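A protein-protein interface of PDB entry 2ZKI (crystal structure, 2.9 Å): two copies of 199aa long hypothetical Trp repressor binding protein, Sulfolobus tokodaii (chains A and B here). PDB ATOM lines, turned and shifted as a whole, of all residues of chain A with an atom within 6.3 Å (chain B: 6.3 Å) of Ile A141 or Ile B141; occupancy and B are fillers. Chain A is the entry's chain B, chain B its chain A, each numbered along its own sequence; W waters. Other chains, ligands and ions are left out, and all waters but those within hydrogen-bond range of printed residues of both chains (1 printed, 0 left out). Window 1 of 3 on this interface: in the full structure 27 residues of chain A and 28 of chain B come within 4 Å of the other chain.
OG of Ser B131 sits close to OH of Tyr A135, at 3.3 Å. The backbone NH (N) of Ile B141 sits at hydrogen-bond distance from the backbone carbonyl oxygen (O) of Ile A141 (2.9 Å).
N of Ile B140 sits at hydrogen-bond distance from O of Lys B108. O of Ile B140 lies within hydrogen-bond range of N of Val B110 (2.8 Å). The backbone carbonyl oxygen of Val B110 sits at hydrogen-bond distance from the backbone NH of Val B142 (2.7 Å). The side-chain hydroxyl (OG1) of Thr B111 sits at hydrogen-bond distance from the backbone carbonyl oxygen (O) of Val B142 (2.8 Å). O of Ile A140 is in hydrogen-bond range of N of Val A110 (2.9 Å). OG1 of Thr A111 is in hydrogen-bond range of O of Val A142, 2.9 Å away.
Tyr B135 touches Ser A131 (OH to CB, 3.2 Å). Tyr A135 touches Ile B141 (OH to CG2, 3.6 Å). Tyr A135 touches Pro B143. Ile A140 touches Ile B141. Pro B143 touches Ile A140. OH of Tyr B135 touches CG2 of Ile A141 (3.5 Å). Ile A141 touches Ile B140. Val A142 touches Ile B140 (CA to CG2, 3.8 Å). Ala B134 touches Pro A143 (O to CG, 3.7 Å). Tyr B135 touches Pro A143.
Of the printed residues of chain B, Ile A141 touches Tyr B135, Ile B140 and Ile B141. Of the printed residues of chain A, Val B142 touches Ile A140. Of the printed residues of chain B, Ile A140 touches Ile B141, Val B142 and Pro B143. The nearest printed residue of chain B that does not touch Tyr A135 is Phe B112 (5.1 Å).
Hydrophobic or aromatic side chains of chain A within 4 Å of the printed part of chain B: Tyr A135, Ile A140, Ile A141, Val A142 and Pro A143. Of the 14 printed residues of chain B, 8 touch a printed residue of chain A.
Ser A131 touches Tyr B135, and with the chains exchanged Tyr A135 touches Ser B131. Tyr A135 touches Ile B141, and with the chains exchanged Ile A141 touches Tyr B135. Tyr A135 touches Pro B143, and with the chains exchanged Pro A143 touches Tyr B135. Pro A143 touches Ala B134, but with the chains exchanged Ala A134 does not touch Pro B143 (4.02 Å).
Water W1 lies within hydrogen-bond range of the side-chain hydroxyl (OH) of Tyr B135 (2.8 Å), the side-chain hydroxyl (OH) of Tyr A135 (2.9 Å), the side-chain hydroxyl (OG) of Ser B131 (2.9 Å) and the side-chain hydroxyl (OG) of Ser A131 (2.9 Å).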
ATOM      1  N   LYS A 108       5.671  11.068 -17.159  1.00  0.00           N
ATOM      2  CA  LYS A 108       4.657  10.554 -18.074  1.00  0.00           C
ATOM      3  C   LYS A 108       4.597   9.025 -18.059  1.00  0.00           C
ATOM      4  O   LYS A 108       5.634   8.366 -18.139  1.00  0.00           O
ATOM      5  CB  LYS A 108       4.886  11.090 -19.492  1.00  0.00           C
ATOM      6  CG  LYS A 108       4.587  12.580 -19.630  1.00  0.00           C
ATOM      7  CD  LYS A 108       4.408  13.017 -21.079  1.00  0.00           C
ATOM      8  CE  LYS A 108       5.733  13.393 -21.738  1.00  0.00           C
ATOM      9  NZ  LYS A 108       5.536  14.141 -23.019  1.00  0.00           N
ATOM     10  N   PRO A 109       3.379   8.459 -17.940  1.00  0.00           N
ATOM     11  CA  PRO A 109       3.143   7.014 -17.865  1.00  0.00           C
ATOM     12  C   PRO A 109       3.623   6.232 -19.086  1.00  0.00           C
ATOM     13  O   PRO A 109       3.617   6.749 -20.207  1.00  0.00           O
ATOM     14  CB  PRO A 109       1.616   6.913 -17.767  1.00  0.00           C
ATOM     15  CG  PRO A 109       1.172   8.221 -17.258  1.00  0.00           C
ATOM     16  CD  PRO A 109       2.116   9.212 -17.851  1.00  0.00           C
ATOM     17  N   VAL A 110       4.028   4.987 -18.853  1.00  0.00           N
ATOM     18  CA  VAL A 110       4.419   4.075 -19.926  1.00  0.00           C
ATOM     19  C   VAL A 110       3.946   2.650 -19.621  1.00  0.00           C
ATOM     20  O   VAL A 110       3.947   2.218 -18.466  1.00  0.00           O
ATOM     21  CB  VAL A 110       5.955   4.127 -20.209  1.00  0.00           C
ATOM     22  CG1 VAL A 110       6.770   3.716 -18.980  1.00  0.00           C
ATOM     23  CG2 VAL A 110       6.321   3.285 -21.429  1.00  0.00           C
ATOM     24  N   THR A 111       3.514   1.945 -20.661  1.00  0.00           N
ATOM     25  CA  THR A 111       3.142   0.539 -20.548  1.00  0.00           C
ATOM     26  C   THR A 111       3.811  -0.264 -21.663  1.00  0.00           C
ATOM     27  O   THR A 111       3.990   0.235 -22.779  1.00  0.00           O
ATOM     28  CB  THR A 111       1.603   0.340 -20.539  1.00  0.00           C
ATOM     29  OG1 THR A 111       1.298  -1.023 -20.218  1.00  0.00           O
ATOM     30  CG2 THR A 111       0.975   0.705 -21.884  1.00  0.00           C
ATOM     31  N   PHE A 112       4.194  -1.499 -21.357  1.00  0.00           N
ATOM     32  CA  PHE A 112       4.997  -2.287 -22.286  1.00  0.00           C
ATOM     33  C   PHE A 112       4.279  -3.548 -22.742  1.00  0.00           C
ATOM     34  O   PHE A 112       3.549  -4.168 -21.967  1.00  0.00           O
ATOM     35  CB  PHE A 112       6.339  -2.663 -21.651  1.00  0.00           C
ATOM     36  CG  PHE A 112       7.105  -1.498 -21.095  1.00  0.00           C
ATOM     37  CD1 PHE A 112       7.040  -1.189 -19.740  1.00  0.00           C
ATOM     38  CD2 PHE A 112       7.908  -0.717 -21.920  1.00  0.00           C
ATOM     39  CE1 PHE A 112       7.756  -0.113 -19.214  1.00  0.00           C
ATOM     40  CE2 PHE A 112       8.630   0.362 -21.403  1.00  0.00           C
ATOM     41  CZ  PHE A 112       8.553   0.662 -20.047  1.00  0.00           C
ATOM     42  N   SER A 131      11.699  -2.037 -19.058  1.00  0.00           N
ATOM     43  CA  SER A 131      11.251  -1.095 -18.034  1.00  0.00           C
ATOM     44  C   SER A 131      12.358  -0.178 -17.515  1.00  0.00           C
ATOM     45  O   SER A 131      12.072   0.864 -16.926  1.00  0.00           O
ATOM     46  CB  SER A 131      10.558  -1.821 -16.877  1.00  0.00           C
ATOM     47  OG  SER A 131      11.490  -2.413 -15.992  1.00  0.00           O
ATOM     48  N   THR A 132      13.613  -0.562 -17.743  1.00  0.00           N
ATOM     49  CA  THR A 132      14.763   0.208 -17.261  1.00  0.00           C
ATOM     50  C   THR A 132      14.779   1.624 -17.833  1.00  0.00           C
ATOM     51  O   THR A 132      15.082   2.583 -17.119  1.00  0.00           O
ATOM     52  CB  THR A 132      16.102  -0.496 -17.565  1.00  0.00           C
ATOM     53  OG1 THR A 132      16.193  -0.785 -18.965  1.00  0.00           O
ATOM     54  CG2 THR A 132      16.223  -1.787 -16.768  1.00  0.00           C
ATOM     55  N   ALA A 134      12.320   3.561 -18.512  1.00  0.00           N
ATOM     56  CA  ALA A 134      11.417   4.397 -17.727  1.00  0.00           C
ATOM     57  C   ALA A 134      12.078   4.967 -16.471  1.00  0.00           C
ATOM     58  O   ALA A 134      11.811   6.109 -16.097  1.00  0.00           O
ATOM     59  CB  ALA A 134      10.163   3.628 -17.365  1.00  0.00           C
ATOM     60  N   TYR A 135      12.940   4.173 -15.836  1.00  0.00           N
ATOM     61  CA  TYR A 135      13.626   4.591 -14.613  1.00  0.00           C
ATOM     62  C   TYR A 135      14.559   5.770 -14.850  1.00  0.00           C
ATOM     63  O   TYR A 135      14.560   6.726 -14.077  1.00  0.00           O
ATOM     64  CB  TYR A 135      14.407   3.432 -13.991  1.00  0.00           C
ATOM     65  CG  TYR A 135      13.545   2.378 -13.334  1.00  0.00           C
ATOM     66  CD1 TYR A 135      13.199   1.216 -14.016  1.00  0.00           C
ATOM     67  CD2 TYR A 135      13.086   2.537 -12.024  1.00  0.00           C
ATOM     68  CE1 TYR A 135      12.414   0.237 -13.418  1.00  0.00           C
ATOM     69  CE2 TYR A 135      12.297   1.566 -11.415  1.00  0.00           C
ATOM     70  CZ  TYR A 135      11.965   0.418 -12.121  1.00  0.00           C
ATOM     71  OH  TYR A 135      11.186  -0.550 -11.537  1.00  0.00           O
ATOM     72  N   MET A 139       9.918   8.130 -15.939  1.00  0.00           N
ATOM     73  CA  MET A 139       8.577   7.777 -16.396  1.00  0.00           C
ATOM     74  C   MET A 139       7.986   6.710 -15.490  1.00  0.00           C
ATOM     75  O   MET A 139       8.668   5.756 -15.125  1.00  0.00           O
ATOM     76  CB  MET A 139       8.620   7.245 -17.828  1.00  0.00           C
ATOM     77  CG  MET A 139       9.243   8.188 -18.839  1.00  0.00           C
ATOM     78  SD  MET A 139       9.412   7.410 -20.451  1.00  0.00           S
ATOM     79  CE  MET A 139       7.721   7.492 -21.020  1.00  0.00           C
ATOM     80  N   ILE A 140       6.714   6.867 -15.140  1.00  0.00           N
ATOM     81  CA  ILE A 140       6.047   5.908 -14.262  1.00  0.00           C
ATOM     82  C   ILE A 140       5.549   4.688 -15.037  1.00  0.00           C
ATOM     83  O   ILE A 140       4.893   4.822 -16.071  1.00  0.00           O
ATOM     84  CB  ILE A 140       4.923   6.558 -13.402  1.00  0.00           C
ATOM     85  CG1 ILE A 140       3.898   7.295 -14.270  1.00  0.00           C
ATOM     86  CG2 ILE A 140       5.529   7.505 -12.369  1.00  0.00           C
ATOM     87  CD1 ILE A 140       2.651   7.743 -13.515  1.00  0.00           C
ATOM     88  N   ILE A 141       5.882   3.501 -14.536  1.00  0.00           N
ATOM     89  CA  ILE A 141       5.538   2.252 -15.219  1.00  0.00           C
ATOM     90  C   ILE A 141       4.134   1.776 -14.838  1.00  0.00           C
ATOM     91  O   ILE A 141       3.795   1.701 -13.657  1.00  0.00           O
ATOM     92  CB  ILE A 141       6.581   1.138 -14.950  1.00  0.00           C
ATOM     93  CG1 ILE A 141       8.002   1.669 -15.163  1.00  0.00           C
ATOM     94  CG2 ILE A 141       6.319  -0.076 -15.845  1.00  0.00           C
ATOM     95  CD1 ILE A 141       9.084   0.801 -14.577  1.00  0.00           C
ATOM     96  N   VAL A 142       3.334   1.461 -15.855  1.00  0.00           N
ATOM     97  CA  VAL A 142       1.957   1.004 -15.675  1.00  0.00           C
ATOM     98  C   VAL A 142       1.794  -0.454 -16.133  1.00  0.00           C
ATOM     99  O   VAL A 142       1.710  -0.728 -17.333  1.00  0.00           O
ATOM    100  CB  VAL A 142       0.949   1.921 -16.429  1.00  0.00           C
ATOM    101  CG1 VAL A 142      -0.491   1.522 -16.120  1.00  0.00           C
ATOM    102  CG2 VAL A 142       1.179   3.385 -16.077  1.00  0.00           C
ATOM    103  N   PRO A 143       1.775  -1.399 -15.178  1.00  0.00           N
ATOM    104  CA  PRO A 143       1.489  -2.798 -15.489  1.00  0.00           C
ATOM    105  C   PRO A 143      -0.004  -3.063 -15.650  1.00  0.00           C
ATOM    106  O   PRO A 143      -0.831  -2.271 -15.194  1.00  0.00           O
ATOM    107  CB  PRO A 143       2.009  -3.552 -14.256  1.00  0.00           C
ATOM    108  CG  PRO A 143       2.672  -2.525 -13.382  1.00  0.00           C
ATOM    109  CD  PRO A 143       2.067  -1.217 -13.749  1.00  0.00           C
ATOM    110  N   LYS B 108      -2.457   1.623  -7.389  1.00  0.00           N
ATOM    111  CA  LYS B 108      -1.737   2.470  -6.436  1.00  0.00           C
ATOM    112  C   LYS B 108      -0.264   2.623  -6.825  1.00  0.00           C
ATOM    113  O   LYS B 108       0.351   1.672  -7.306  1.00  0.00           O
ATOM    114  CB  LYS B 108      -1.851   1.912  -5.008  1.00  0.00           C
ATOM    115  CG  LYS B 108      -3.276   1.641  -4.516  1.00  0.00           C
ATOM    116  CD  LYS B 108      -4.008   2.910  -4.092  1.00  0.00           C
ATOM    117  CE  LYS B 108      -5.437   2.607  -3.651  1.00  0.00           C
ATOM    118  NZ  LYS B 108      -5.493   1.700  -2.465  1.00  0.00           N
ATOM    119  N   PRO B 109       0.304   3.830  -6.630  1.00  0.00           N
ATOM    120  CA  PRO B 109       1.722   4.060  -6.914  1.00  0.00           C
ATOM    121  C   PRO B 109       2.670   3.487  -5.856  1.00  0.00           C
ATOM    122  O   PRO B 109       2.356   3.493  -4.663  1.00  0.00           O
ATOM    123  CB  PRO B 109       1.824   5.585  -6.949  1.00  0.00           C
ATOM    124  CG  PRO B 109       0.756   6.043  -6.032  1.00  0.00           C
ATOM    125  CD  PRO B 109      -0.367   5.058  -6.166  1.00  0.00           C
ATOM    126  N   VAL B 110       3.823   3.002  -6.310  1.00  0.00           N
ATOM    127  CA  VAL B 110       4.849   2.448  -5.432  1.00  0.00           C
ATOM    128  C   VAL B 110       6.240   2.915  -5.867  1.00  0.00           C
ATOM    129  O   VAL B 110       6.548   2.954  -7.061  1.00  0.00           O
ATOM    130  CB  VAL B 110       4.768   0.883  -5.346  1.00  0.00           C
ATOM    131  CG1 VAL B 110       4.930   0.227  -6.719  1.00  0.00           C
ATOM    132  CG2 VAL B 110       5.781   0.326  -4.352  1.00  0.00           C
ATOM    133  N   THR B 111       7.061   3.286  -4.890  1.00  0.00           N
ATOM    134  CA  THR B 111       8.450   3.660  -5.141  1.00  0.00           C
ATOM    135  C   THR B 111       9.393   2.821  -4.271  1.00  0.00           C
ATOM    136  O   THR B 111       9.024   2.401  -3.170  1.00  0.00           O
ATOM    137  CB  THR B 111       8.693   5.189  -4.952  1.00  0.00           C
ATOM    138  OG1 THR B 111      10.007   5.531  -5.406  1.00  0.00           O
ATOM    139  CG2 THR B 111       8.525   5.617  -3.494  1.00  0.00           C
ATOM    140  N   PHE B 112      10.602   2.576  -4.773  1.00  0.00           N
ATOM    141  CA  PHE B 112      11.543   1.687  -4.097  1.00  0.00           C
ATOM    142  C   PHE B 112      12.848   2.371  -3.721  1.00  0.00           C
ATOM    143  O   PHE B 112      13.348   3.235  -4.447  1.00  0.00           O
ATOM    144  CB  PHE B 112      11.839   0.454  -4.955  1.00  0.00           C
ATOM    145  CG  PHE B 112      10.618  -0.334  -5.330  1.00  0.00           C
ATOM    146  CD1 PHE B 112      10.059  -0.207  -6.596  1.00  0.00           C
ATOM    147  CD2 PHE B 112      10.029  -1.204  -4.419  1.00  0.00           C
ATOM    148  CE1 PHE B 112       8.928  -0.934  -6.952  1.00  0.00           C
ATOM    149  CE2 PHE B 112       8.900  -1.937  -4.761  1.00  0.00           C
ATOM    150  CZ  PHE B 112       8.348  -1.805  -6.030  1.00  0.00           C
ATOM    151  N   SER B 131      10.647  -4.659  -8.023  1.00  0.00           N
ATOM    152  CA  SER B 131       9.554  -4.063  -8.785  1.00  0.00           C
ATOM    153  C   SER B 131       8.598  -5.081  -9.395  1.00  0.00           C
ATOM    154  O   SER B 131       7.478  -4.729  -9.761  1.00  0.00           O
ATOM    155  CB  SER B 131      10.091  -3.113  -9.859  1.00  0.00           C
ATOM    156  OG  SER B 131      10.898  -3.794 -10.799  1.00  0.00           O
ATOM    157  N   THR B 132       9.030  -6.339  -9.486  1.00  0.00           N
ATOM    158  CA  THR B 132       8.187  -7.410 -10.040  1.00  0.00           C
ATOM    159  C   THR B 132       6.886  -7.574  -9.249  1.00  0.00           C
ATOM    160  O   THR B 132       5.858  -7.972  -9.803  1.00  0.00           O
ATOM    161  CB  THR B 132       8.926  -8.766 -10.115  1.00  0.00           C
ATOM    162  OG1 THR B 132       9.453  -9.099  -8.826  1.00  0.00           O
ATOM    163  CG2 THR B 132      10.060  -8.713 -11.124  1.00  0.00           C
ATOM    164  N   ALA B 134       5.055  -5.153  -8.114  1.00  0.00           N
ATOM    165  CA  ALA B 134       4.114  -4.163  -8.630  1.00  0.00           C
ATOM    166  C   ALA B 134       3.365  -4.626  -9.876  1.00  0.00           C
ATOM    167  O   ALA B 134       2.223  -4.226 -10.101  1.00  0.00           O
ATOM    168  CB  ALA B 134       4.831  -2.857  -8.901  1.00  0.00           C
ATOM    169  N   TYR B 135       4.008  -5.464 -10.684  1.00  0.00           N
ATOM    170  CA  TYR B 135       3.390  -5.986 -11.899  1.00  0.00           C
ATOM    171  C   TYR B 135       2.262  -6.969 -11.594  1.00  0.00           C
ATOM    172  O   TYR B 135       1.211  -6.930 -12.227  1.00  0.00           O
ATOM    173  CB  TYR B 135       4.439  -6.639 -12.803  1.00  0.00           C
ATOM    174  CG  TYR B 135       5.428  -5.662 -13.397  1.00  0.00           C
ATOM    175  CD1 TYR B 135       6.588  -5.310 -12.709  1.00  0.00           C
ATOM    176  CD2 TYR B 135       5.209  -5.093 -14.649  1.00  0.00           C
ATOM    177  CE1 TYR B 135       7.500  -4.415 -13.247  1.00  0.00           C
ATOM    178  CE2 TYR B 135       6.113  -4.192 -15.196  1.00  0.00           C
ATOM    179  CZ  TYR B 135       7.257  -3.858 -14.491  1.00  0.00           C
ATOM    180  OH  TYR B 135       8.158  -2.972 -15.027  1.00  0.00           O
ATOM    181  N   MET B 139       0.130  -2.590  -9.446  1.00  0.00           N
ATOM    182  CA  MET B 139       0.590  -1.320  -8.887  1.00  0.00           C
ATOM    183  C   MET B 139       1.501  -0.580  -9.861  1.00  0.00           C
ATOM    184  O   MET B 139       2.298  -1.204 -10.565  1.00  0.00           O
ATOM    185  CB  MET B 139       1.337  -1.564  -7.577  1.00  0.00           C
ATOM    186  CG  MET B 139       0.489  -2.203  -6.492  1.00  0.00           C
ATOM    187  SD  MET B 139       1.438  -2.638  -5.031  1.00  0.00           S
ATOM    188  CE  MET B 139       1.731  -1.023  -4.317  1.00  0.00           C
ATOM    189  N   ILE B 140       1.388   0.746  -9.898  1.00  0.00           N
ATOM    190  CA  ILE B 140       2.218   1.561 -10.794  1.00  0.00           C
ATOM    191  C   ILE B 140       3.531   2.008 -10.138  1.00  0.00           C
ATOM    192  O   ILE B 140       3.535   2.500  -9.012  1.00  0.00           O
ATOM    193  CB  ILE B 140       1.440   2.764 -11.402  1.00  0.00           C
ATOM    194  CG1 ILE B 140       0.776   3.607 -10.312  1.00  0.00           C
ATOM    195  CG2 ILE B 140       0.402   2.266 -12.410  1.00  0.00           C
ATOM    196  CD1 ILE B 140       0.286   4.968 -10.789  1.00  0.00           C
ATOM    197  N   ILE B 141       4.638   1.823 -10.855  1.00  0.00           N
ATOM    198  CA  ILE B 141       5.980   2.100 -10.331  1.00  0.00           C
ATOM    199  C   ILE B 141       6.369   3.564 -10.521  1.00  0.00           C
ATOM    200  O   ILE B 141       6.234   4.108 -11.613  1.00  0.00           O
ATOM    201  CB  ILE B 141       7.047   1.190 -11.002  1.00  0.00           C
ATOM    202  CG1 ILE B 141       6.679  -0.286 -10.829  1.00  0.00           C
ATOM    203  CG2 ILE B 141       8.443   1.465 -10.437  1.00  0.00           C
ATOM    204  CD1 ILE B 141       7.260  -1.195 -11.885  1.00  0.00           C
ATOM    205  N   VAL B 142       6.856   4.189  -9.451  1.00  0.00           N
ATOM    206  CA  VAL B 142       7.320   5.577  -9.502  1.00  0.00           C
ATOM    207  C   VAL B 142       8.839   5.664  -9.289  1.00  0.00           C
ATOM    208  O   VAL B 142       9.323   5.583  -8.154  1.00  0.00           O
ATOM    209  CB  VAL B 142       6.576   6.475  -8.473  1.00  0.00           C
ATOM    210  CG1 VAL B 142       7.113   7.904  -8.505  1.00  0.00           C
ATOM    211  CG2 VAL B 142       5.074   6.468  -8.737  1.00  0.00           C
ATOM    212  N   PRO B 143       9.600   5.803 -10.387  1.00  0.00           N
ATOM    213  CA  PRO B 143      11.026   6.102 -10.274  1.00  0.00           C
ATOM    214  C   PRO B 143      11.238   7.584  -9.982  1.00  0.00           C
ATOM    215  O   PRO B 143      10.325   8.385 -10.184  1.00  0.00           O
ATOM    216  CB  PRO B 143      11.572   5.767 -11.671  1.00  0.00           C
ATOM    217  CG  PRO B 143      10.422   5.168 -12.439  1.00  0.00           C
ATOM    218  CD  PRO B 143       9.184   5.668 -11.792  1.00  0.00           C
HETATM  219  O   HOH W   1      10.286  -2.590 -13.318  1.00  0.00           O
